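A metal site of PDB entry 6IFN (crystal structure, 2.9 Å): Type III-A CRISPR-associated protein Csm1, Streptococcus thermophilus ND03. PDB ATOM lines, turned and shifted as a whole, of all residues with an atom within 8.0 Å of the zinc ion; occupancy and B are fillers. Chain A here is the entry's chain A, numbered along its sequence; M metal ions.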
ATOM      1  N   PHE A 254     -33.884   0.138  15.272  1.00  0.00           N
ATOM      2  CA  PHE A 254     -32.595   0.737  15.630  1.00  0.00           C
ATOM      3  C   PHE A 254     -32.757   1.910  16.596  1.00  0.00           C
ATOM      4  O   PHE A 254     -32.000   2.038  17.534  1.00  0.00           O
ATOM      5  CB  PHE A 254     -31.904   1.260  14.380  1.00  0.00           C
ATOM      6  CG  PHE A 254     -30.563   1.903  14.637  1.00  0.00           C
ATOM      7  CD1 PHE A 254     -30.468   3.257  14.889  1.00  0.00           C
ATOM      8  CD2 PHE A 254     -29.394   1.164  14.578  1.00  0.00           C
ATOM      9  CE1 PHE A 254     -29.240   3.860  15.085  1.00  0.00           C
ATOM     10  CE2 PHE A 254     -28.151   1.760  14.789  1.00  0.00           C
ATOM     11  CZ  PHE A 254     -28.088   3.110  15.050  1.00  0.00           C
ATOM     12  N   ASN A 257     -34.717   0.512  20.066  1.00  0.00           N
ATOM     13  CA  ASN A 257     -34.107  -0.575  20.876  1.00  0.00           C
ATOM     14  C   ASN A 257     -32.989  -0.053  21.792  1.00  0.00           C
ATOM     15  O   ASN A 257     -31.796  -0.076  21.468  1.00  0.00           O
ATOM     16  CB  ASN A 257     -33.534  -1.707  20.023  1.00  0.00           C
ATOM     17  CG  ASN A 257     -32.999  -2.796  20.916  1.00  0.00           C
ATOM     18  OD1 ASN A 257     -31.790  -3.016  20.986  1.00  0.00           O
ATOM     19  ND2 ASN A 257     -33.939  -3.419  21.622  1.00  0.00           N
ATOM     20  N   ILE A 258     -33.389   0.432  22.965  1.00  0.00           N
ATOM     21  CA  ILE A 258     -32.503   0.857  23.977  1.00  0.00           C
ATOM     22  C   ILE A 258     -32.747  -0.045  25.168  1.00  0.00           C
ATOM     23  O   ILE A 258     -33.881  -0.172  25.604  1.00  0.00           O
ATOM     24  CB  ILE A 258     -32.735   2.340  24.328  1.00  0.00           C
ATOM     25  CG1 ILE A 258     -32.333   3.280  23.190  1.00  0.00           C
ATOM     26  CG2 ILE A 258     -32.045   2.700  25.640  1.00  0.00           C
ATOM     27  CD1 ILE A 258     -31.150   2.826  22.358  1.00  0.00           C
ATOM     28  N   GLN A 268     -29.608   8.941  23.723  1.00  0.00           N
ATOM     29  CA  GLN A 268     -29.477   8.057  22.567  1.00  0.00           C
ATOM     30  C   GLN A 268     -30.765   8.026  21.717  1.00  0.00           C
ATOM     31  O   GLN A 268     -30.683   7.813  20.527  1.00  0.00           O
ATOM     32  CB  GLN A 268     -29.192   6.630  23.003  1.00  0.00           C
ATOM     33  CG  GLN A 268     -27.829   6.427  23.642  1.00  0.00           C
ATOM     34  CD  GLN A 268     -26.785   6.109  22.617  1.00  0.00           C
ATOM     35  OE1 GLN A 268     -27.079   5.598  21.530  1.00  0.00           O
ATOM     36  NE2 GLN A 268     -25.541   6.406  22.950  1.00  0.00           N
ATOM     37  N   ARG A 272     -30.391   8.937  17.925  1.00  0.00           N
ATOM     38  CA  ARG A 272     -30.622   7.885  16.947  1.00  0.00           C
ATOM     39  C   ARG A 272     -31.627   8.359  15.901  1.00  0.00           C
ATOM     40  O   ARG A 272     -31.441   8.157  14.696  1.00  0.00           O
ATOM     41  CB  ARG A 272     -31.133   6.630  17.657  1.00  0.00           C
ATOM     42  CG  ARG A 272     -30.041   5.901  18.424  1.00  0.00           C
ATOM     43  CD  ARG A 272     -30.448   4.815  19.385  1.00  0.00           C
ATOM     44  NE  ARG A 272     -29.278   4.009  19.745  1.00  0.00           N
ATOM     45  CZ  ARG A 272     -28.832   2.939  19.069  1.00  0.00           C
ATOM     46  NH1 ARG A 272     -29.434   2.529  17.971  1.00  0.00           N
ATOM     47  NH2 ARG A 272     -27.764   2.289  19.484  1.00  0.00           N
ATOM     48  N   ARG A 338     -28.311  -4.741  10.813  1.00  0.00           N
ATOM     49  CA  ARG A 338     -29.269  -3.798  11.424  1.00  0.00           C
ATOM     50  C   ARG A 338     -29.837  -2.766  10.435  1.00  0.00           C
ATOM     51  O   ARG A 338     -30.944  -2.359  10.647  1.00  0.00           O
ATOM     52  CB  ARG A 338     -28.731  -3.253  12.740  1.00  0.00           C
ATOM     53  CG  ARG A 338     -28.380  -4.360  13.709  1.00  0.00           C
ATOM     54  CD  ARG A 338     -28.346  -3.838  15.116  1.00  0.00           C
ATOM     55  NE  ARG A 338     -27.317  -2.841  15.259  1.00  0.00           N
ATOM     56  CZ  ARG A 338     -26.165  -3.019  15.876  1.00  0.00           C
ATOM     57  NH1 ARG A 338     -25.316  -2.027  15.979  1.00  0.00           N
ATOM     58  NH2 ARG A 338     -25.874  -4.197  16.389  1.00  0.00           N
ATOM     59  N   GLU A 400     -20.513  -7.118  26.128  1.00  0.00           N
ATOM     60  CA  GLU A 400     -21.234  -6.569  24.979  1.00  0.00           C
ATOM     61  C   GLU A 400     -21.656  -5.137  25.298  1.00  0.00           C
ATOM     62  O   GLU A 400     -21.573  -4.731  26.443  1.00  0.00           O
ATOM     63  CB  GLU A 400     -22.444  -7.455  24.696  1.00  0.00           C
ATOM     64  CG  GLU A 400     -23.528  -7.321  25.742  1.00  0.00           C
ATOM     65  CD  GLU A 400     -24.429  -8.534  25.855  1.00  0.00           C
ATOM     66  OE1 GLU A 400     -24.386  -9.369  24.964  1.00  0.00           O
ATOM     67  OE2 GLU A 400     -25.170  -8.625  26.832  1.00  0.00           O
ATOM     68  N   CYS A 401     -22.130  -4.381  24.296  1.00  0.00           N
ATOM     69  CA  CYS A 401     -22.574  -3.019  24.528  1.00  0.00           C
ATOM     70  C   CYS A 401     -23.900  -3.034  25.275  1.00  0.00           C
ATOM     71  O   CYS A 401     -24.844  -3.635  24.777  1.00  0.00           O
ATOM     72  CB  CYS A 401     -22.745  -2.285  23.206  1.00  0.00           C
ATOM     73  SG  CYS A 401     -23.801  -0.820  23.261  1.00  0.00           S
ATOM     74  N   GLU A 402     -23.968  -2.358  26.428  1.00  0.00           N
ATOM     75  CA  GLU A 402     -25.177  -2.446  27.296  1.00  0.00           C
ATOM     76  C   GLU A 402     -26.392  -1.909  26.546  1.00  0.00           C
ATOM     77  O   GLU A 402     -27.478  -2.376  26.793  1.00  0.00           O
ATOM     78  CB  GLU A 402     -25.029  -1.688  28.609  1.00  0.00           C
ATOM     79  CG  GLU A 402     -24.689  -0.221  28.427  1.00  0.00           C
ATOM     80  CD  GLU A 402     -24.809   0.616  29.693  1.00  0.00           C
ATOM     81  OE1 GLU A 402     -24.964  -0.003  30.786  1.00  0.00           O
ATOM     82  OE2 GLU A 402     -24.740   1.893  29.573  1.00  0.00           O
ATOM     83  N   ILE A 403     -26.190  -0.974  25.608  1.00  0.00           N
ATOM     84  CA  ILE A 403     -27.252  -0.345  24.870  1.00  0.00           C
ATOM     85  C   ILE A 403     -27.834  -1.358  23.880  1.00  0.00           C
ATOM     86  O   ILE A 403     -28.990  -1.734  24.020  1.00  0.00           O
ATOM     87  CB  ILE A 403     -26.789   0.965  24.193  1.00  0.00           C
ATOM     88  CG1 ILE A 403     -25.897   1.847  25.080  1.00  0.00           C
ATOM     89  CG2 ILE A 403     -27.983   1.762  23.695  1.00  0.00           C
ATOM     90  CD1 ILE A 403     -26.630   2.585  26.202  1.00  0.00           C
ATOM     91  N   CYS A 404     -27.034  -1.833  22.893  1.00  0.00           N
ATOM     92  CA  CYS A 404     -27.554  -2.567  21.697  1.00  0.00           C
ATOM     93  C   CYS A 404     -27.137  -4.041  21.625  1.00  0.00           C
ATOM     94  O   CYS A 404     -27.487  -4.745  20.694  1.00  0.00           O
ATOM     95  CB  CYS A 404     -27.069  -1.869  20.432  1.00  0.00           C
ATOM     96  SG  CYS A 404     -25.270  -1.669  20.366  1.00  0.00           S
ATOM     97  N   HIS A 405     -26.350  -4.520  22.588  1.00  0.00           N
ATOM     98  CA  HIS A 405     -25.746  -5.890  22.571  1.00  0.00           C
ATOM     99  C   HIS A 405     -24.725  -6.120  21.446  1.00  0.00           C
ATOM    100  O   HIS A 405     -24.430  -7.268  21.087  1.00  0.00           O
ATOM    101  CB  HIS A 405     -26.805  -6.998  22.507  1.00  0.00           C
ATOM    102  CG  HIS A 405     -27.668  -7.104  23.711  1.00  0.00           C
ATOM    103  ND1 HIS A 405     -27.445  -6.348  24.847  1.00  0.00           N
ATOM    104  CD2 HIS A 405     -28.724  -7.890  23.970  1.00  0.00           C
ATOM    105  CE1 HIS A 405     -28.360  -6.625  25.736  1.00  0.00           C
ATOM    106  NE2 HIS A 405     -29.162  -7.567  25.219  1.00  0.00           N
ATOM    107  N   SER A 406     -24.108  -5.064  20.939  1.00  0.00           N
ATOM    108  CA  SER A 406     -23.053  -5.214  19.964  1.00  0.00           C
ATOM    109  C   SER A 406     -21.781  -5.663  20.675  1.00  0.00           C
ATOM    110  O   SER A 406     -21.517  -5.254  21.814  1.00  0.00           O
ATOM    111  CB  SER A 406     -22.855  -3.928  19.207  1.00  0.00           C
ATOM    112  OG  SER A 406     -21.812  -4.024  18.245  1.00  0.00           O
ATOM    113  N   VAL A 407     -20.978  -6.468  19.977  1.00  0.00           N
ATOM    114  CA  VAL A 407     -19.652  -6.870  20.436  1.00  0.00           C
ATOM    115  C   VAL A 407     -18.573  -6.228  19.555  1.00  0.00           C
ATOM    116  O   VAL A 407     -17.425  -6.641  19.635  1.00  0.00           O
ATOM    117  CB  VAL A 407     -19.477  -8.404  20.442  1.00  0.00           C
ATOM    118  CG1 VAL A 407     -20.286  -9.071  21.539  1.00  0.00           C
ATOM    119  CG2 VAL A 407     -19.831  -8.999  19.097  1.00  0.00           C
ATOM    120  N   GLU A 408     -18.958  -5.247  18.734  1.00  0.00           N
ATOM    121  CA  GLU A 408     -18.088  -4.684  17.732  1.00  0.00           C
ATOM    122  C   GLU A 408     -17.477  -3.381  18.247  1.00  0.00           C
ATOM    123  O   GLU A 408     -18.174  -2.473  18.612  1.00  0.00           O
ATOM    124  CB  GLU A 408     -18.852  -4.445  16.435  1.00  0.00           C
ATOM    125  CG  GLU A 408     -17.958  -4.564  15.217  1.00  0.00           C
ATOM    126  CD  GLU A 408     -17.602  -5.983  14.778  1.00  0.00           C
ATOM    127  OE1 GLU A 408     -18.300  -6.953  15.210  1.00  0.00           O
ATOM    128  OE2 GLU A 408     -16.626  -6.112  13.995  1.00  0.00           O
ATOM    129  N   LEU A 410     -15.902  -2.276  20.981  1.00  0.00           N
ATOM    130  CA  LEU A 410     -16.318  -1.764  22.281  1.00  0.00           C
ATOM    131  C   LEU A 410     -15.358  -0.714  22.805  1.00  0.00           C
ATOM    132  O   LEU A 410     -14.173  -0.691  22.452  1.00  0.00           O
ATOM    133  CB  LEU A 410     -16.434  -2.925  23.269  1.00  0.00           C
ATOM    134  CG  LEU A 410     -17.608  -3.838  22.945  1.00  0.00           C
ATOM    135  CD1 LEU A 410     -18.075  -4.587  24.173  1.00  0.00           C
ATOM    136  CD2 LEU A 410     -18.761  -3.041  22.354  1.00  0.00           C
ATOM    137  N   LYS A 417     -19.960   0.100  29.109  1.00  0.00           N
ATOM    138  CA  LYS A 417     -19.402  -0.483  27.927  1.00  0.00           C
ATOM    139  C   LYS A 417     -20.399  -0.303  26.764  1.00  0.00           C
ATOM    140  O   LYS A 417     -21.559  -0.710  26.861  1.00  0.00           O
ATOM    141  CB  LYS A 417     -19.041  -1.937  28.213  1.00  0.00           C
ATOM    142  CG  LYS A 417     -17.959  -2.484  27.290  1.00  0.00           C
ATOM    143  CD  LYS A 417     -16.793  -3.150  28.002  1.00  0.00           C
ATOM    144  CE  LYS A 417     -15.746  -2.163  28.458  1.00  0.00           C
ATOM    145  NZ  LYS A 417     -14.888  -2.747  29.525  1.00  0.00           N
ATOM    146  N   VAL A 418     -19.928   0.290  25.660  1.00  0.00           N
ATOM    147  CA  VAL A 418     -20.756   0.576  24.531  1.00  0.00           C
ATOM    148  C   VAL A 418     -19.941   0.384  23.268  1.00  0.00           C
ATOM    149  O   VAL A 418     -18.722   0.332  23.371  1.00  0.00           O
ATOM    150  CB  VAL A 418     -21.307   1.997  24.652  1.00  0.00           C
ATOM    151  CG1 VAL A 418     -22.225   2.100  25.853  1.00  0.00           C
ATOM    152  CG2 VAL A 418     -20.228   3.056  24.727  1.00  0.00           C
ATOM    153  N   CYS A 419     -20.601   0.268  22.106  1.00  0.00           N
ATOM    154  CA  CYS A 419     -19.887   0.164  20.791  1.00  0.00           C
ATOM    155  C   CYS A 419     -19.470   1.560  20.343  1.00  0.00           C
ATOM    156  O   CYS A 419     -19.883   2.522  20.988  1.00  0.00           O
ATOM    157  CB  CYS A 419     -20.725  -0.476  19.695  1.00  0.00           C
ATOM    158  SG  CYS A 419     -22.504  -0.146  19.823  1.00  0.00           S
ATOM    159  N   ASP A 420     -18.660   1.660  19.278  1.00  0.00           N
ATOM    160  CA  ASP A 420     -18.220   2.976  18.855  1.00  0.00           C
ATOM    161  C   ASP A 420     -19.403   3.692  18.196  1.00  0.00           C
ATOM    162  O   ASP A 420     -19.422   4.924  18.150  1.00  0.00           O
ATOM    163  CB  ASP A 420     -16.963   2.986  17.963  1.00  0.00           C
ATOM    164  CG  ASP A 420     -16.044   4.178  18.254  1.00  0.00           C
ATOM    165  OD1 ASP A 420     -15.369   4.197  19.335  1.00  0.00           O
ATOM    166  OD2 ASP A 420     -16.011   5.134  17.435  1.00  0.00           O
ATOM    167  N   ILE A 421     -20.371   2.932  17.696  1.00  0.00           N
ATOM    168  CA  ILE A 421     -21.573   3.571  17.200  1.00  0.00           C
ATOM    169  C   ILE A 421     -22.276   4.257  18.361  1.00  0.00           C
ATOM    170  O   ILE A 421     -22.453   5.467  18.312  1.00  0.00           O
ATOM    171  CB  ILE A 421     -22.497   2.573  16.497  1.00  0.00           C
ATOM    172  CG1 ILE A 421     -21.976   2.237  15.110  1.00  0.00           C
ATOM    173  CG2 ILE A 421     -23.894   3.138  16.440  1.00  0.00           C
ATOM    174  CD1 ILE A 421     -21.526   3.453  14.367  1.00  0.00           C
ATOM    175  N   CYS A 422     -22.656   3.487  19.391  1.00  0.00           N
ATOM    176  CA  CYS A 422     -23.371   4.045  20.540  1.00  0.00           C
ATOM    177  C   CYS A 422     -22.548   5.168  21.184  1.00  0.00           C
ATOM    178  O   CYS A 422     -23.119   6.215  21.509  1.00  0.00           O
ATOM    179  CB  CYS A 422     -23.746   2.965  21.540  1.00  0.00           C
ATOM    180  SG  CYS A 422     -24.991   1.798  20.923  1.00  0.00           S
ATOM    181  N   ARG A 423     -21.235   5.000  21.324  1.00  0.00           N
ATOM    182  CA  ARG A 423     -20.390   6.087  21.799  1.00  0.00           C
ATOM    183  C   ARG A 423     -20.636   7.291  20.882  1.00  0.00           C
ATOM    184  O   ARG A 423     -20.945   8.381  21.365  1.00  0.00           O
ATOM    185  CB  ARG A 423     -18.905   5.713  21.878  1.00  0.00           C
ATOM    186  CG  ARG A 423     -18.006   6.824  22.437  1.00  0.00           C
ATOM    187  CD  ARG A 423     -16.817   7.157  21.537  1.00  0.00           C
ATOM    188  NE  ARG A 423     -17.131   7.701  20.194  1.00  0.00           N
ATOM    189  CZ  ARG A 423     -16.898   8.954  19.780  1.00  0.00           C
ATOM    190  NH1 ARG A 423     -16.237   9.812  20.549  1.00  0.00           N
ATOM    191  NH2 ARG A 423     -17.334   9.348  18.587  1.00  0.00           N
ATOM    192  N   LEU A 425     -23.044   8.193  19.136  1.00  0.00           N
ATOM    193  CA  LEU A 425     -24.351   8.776  19.264  1.00  0.00           C
ATOM    194  C   LEU A 425     -24.432   9.562  20.580  1.00  0.00           C
ATOM    195  O   LEU A 425     -25.239  10.492  20.714  1.00  0.00           O
ATOM    196  CB  LEU A 425     -25.424   7.673  19.202  1.00  0.00           C
ATOM    197  CG  LEU A 425     -25.720   7.139  17.798  1.00  0.00           C
ATOM    198  CD1 LEU A 425     -26.474   5.806  17.837  1.00  0.00           C
ATOM    199  CD2 LEU A 425     -26.506   8.154  16.969  1.00  0.00           C
ATOM    200  N   TYR A 426     -23.637   9.158  21.584  1.00  0.00           N
ATOM    201  CA  TYR A 426     -23.534   9.927  22.816  1.00  0.00           C
ATOM    202  C   TYR A 426     -22.905  11.278  22.511  1.00  0.00           C
ATOM    203  O   TYR A 426     -23.334  12.268  23.020  1.00  0.00           O
ATOM    204  CB  TYR A 426     -22.695   9.210  23.848  1.00  0.00           C
ATOM    205  CG  TYR A 426     -23.487   8.291  24.708  1.00  0.00           C
ATOM    206  CD1 TYR A 426     -24.690   8.700  25.275  1.00  0.00           C
ATOM    207  CD2 TYR A 426     -23.034   7.011  24.985  1.00  0.00           C
ATOM    208  CE1 TYR A 426     -25.409   7.848  26.111  1.00  0.00           C
ATOM    209  CE2 TYR A 426     -23.753   6.146  25.802  1.00  0.00           C
ATOM    210  CZ  TYR A 426     -24.937   6.578  26.380  1.00  0.00           C
ATOM    211  OH  TYR A 426     -25.605   5.727  27.182  1.00  0.00           O
HETATM  212 ZN    ZN M   1     -24.117  -0.086  20.951  1.00  0.00          ZN
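N of Ser 406 lies close to SG of Cys 404, at 3.6 Å.
SG of Cys 422 sits close to NH2 of Arg 272, 3.2 Å away.
The backbone carbonyl oxygen (O) of Cys 422 sits at hydrogen-bond distance from the side-chain amide nitrogen (NE2) of Gln 268 (2.8 Å).
The backbone NH (N) of Ile 403 sits close to the side-chain sulfur (SG) of Cys 401 (3.4 Å).
O of Ser 406 sits at hydrogen-bond distance from N of Cys 401, at 2.7 Å.
SG of Cys 419 is bound to the zinc ion.
SG of Cys 404 binds the zinc ion, 2.0 Å away.
SG of Cys 422 is bound to the zinc ion, 2.1 Å away.
The zinc ion is bound by SG of Cys 401, 2.4 Å away.
The zinc ion has four donor atoms within binding distance.
Of the 25 residues printed, 4 come within 4 Å of the zinc ion.
The nearest printed residue that does not touch the zinc ion is Ile 403 (4.3 Å).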
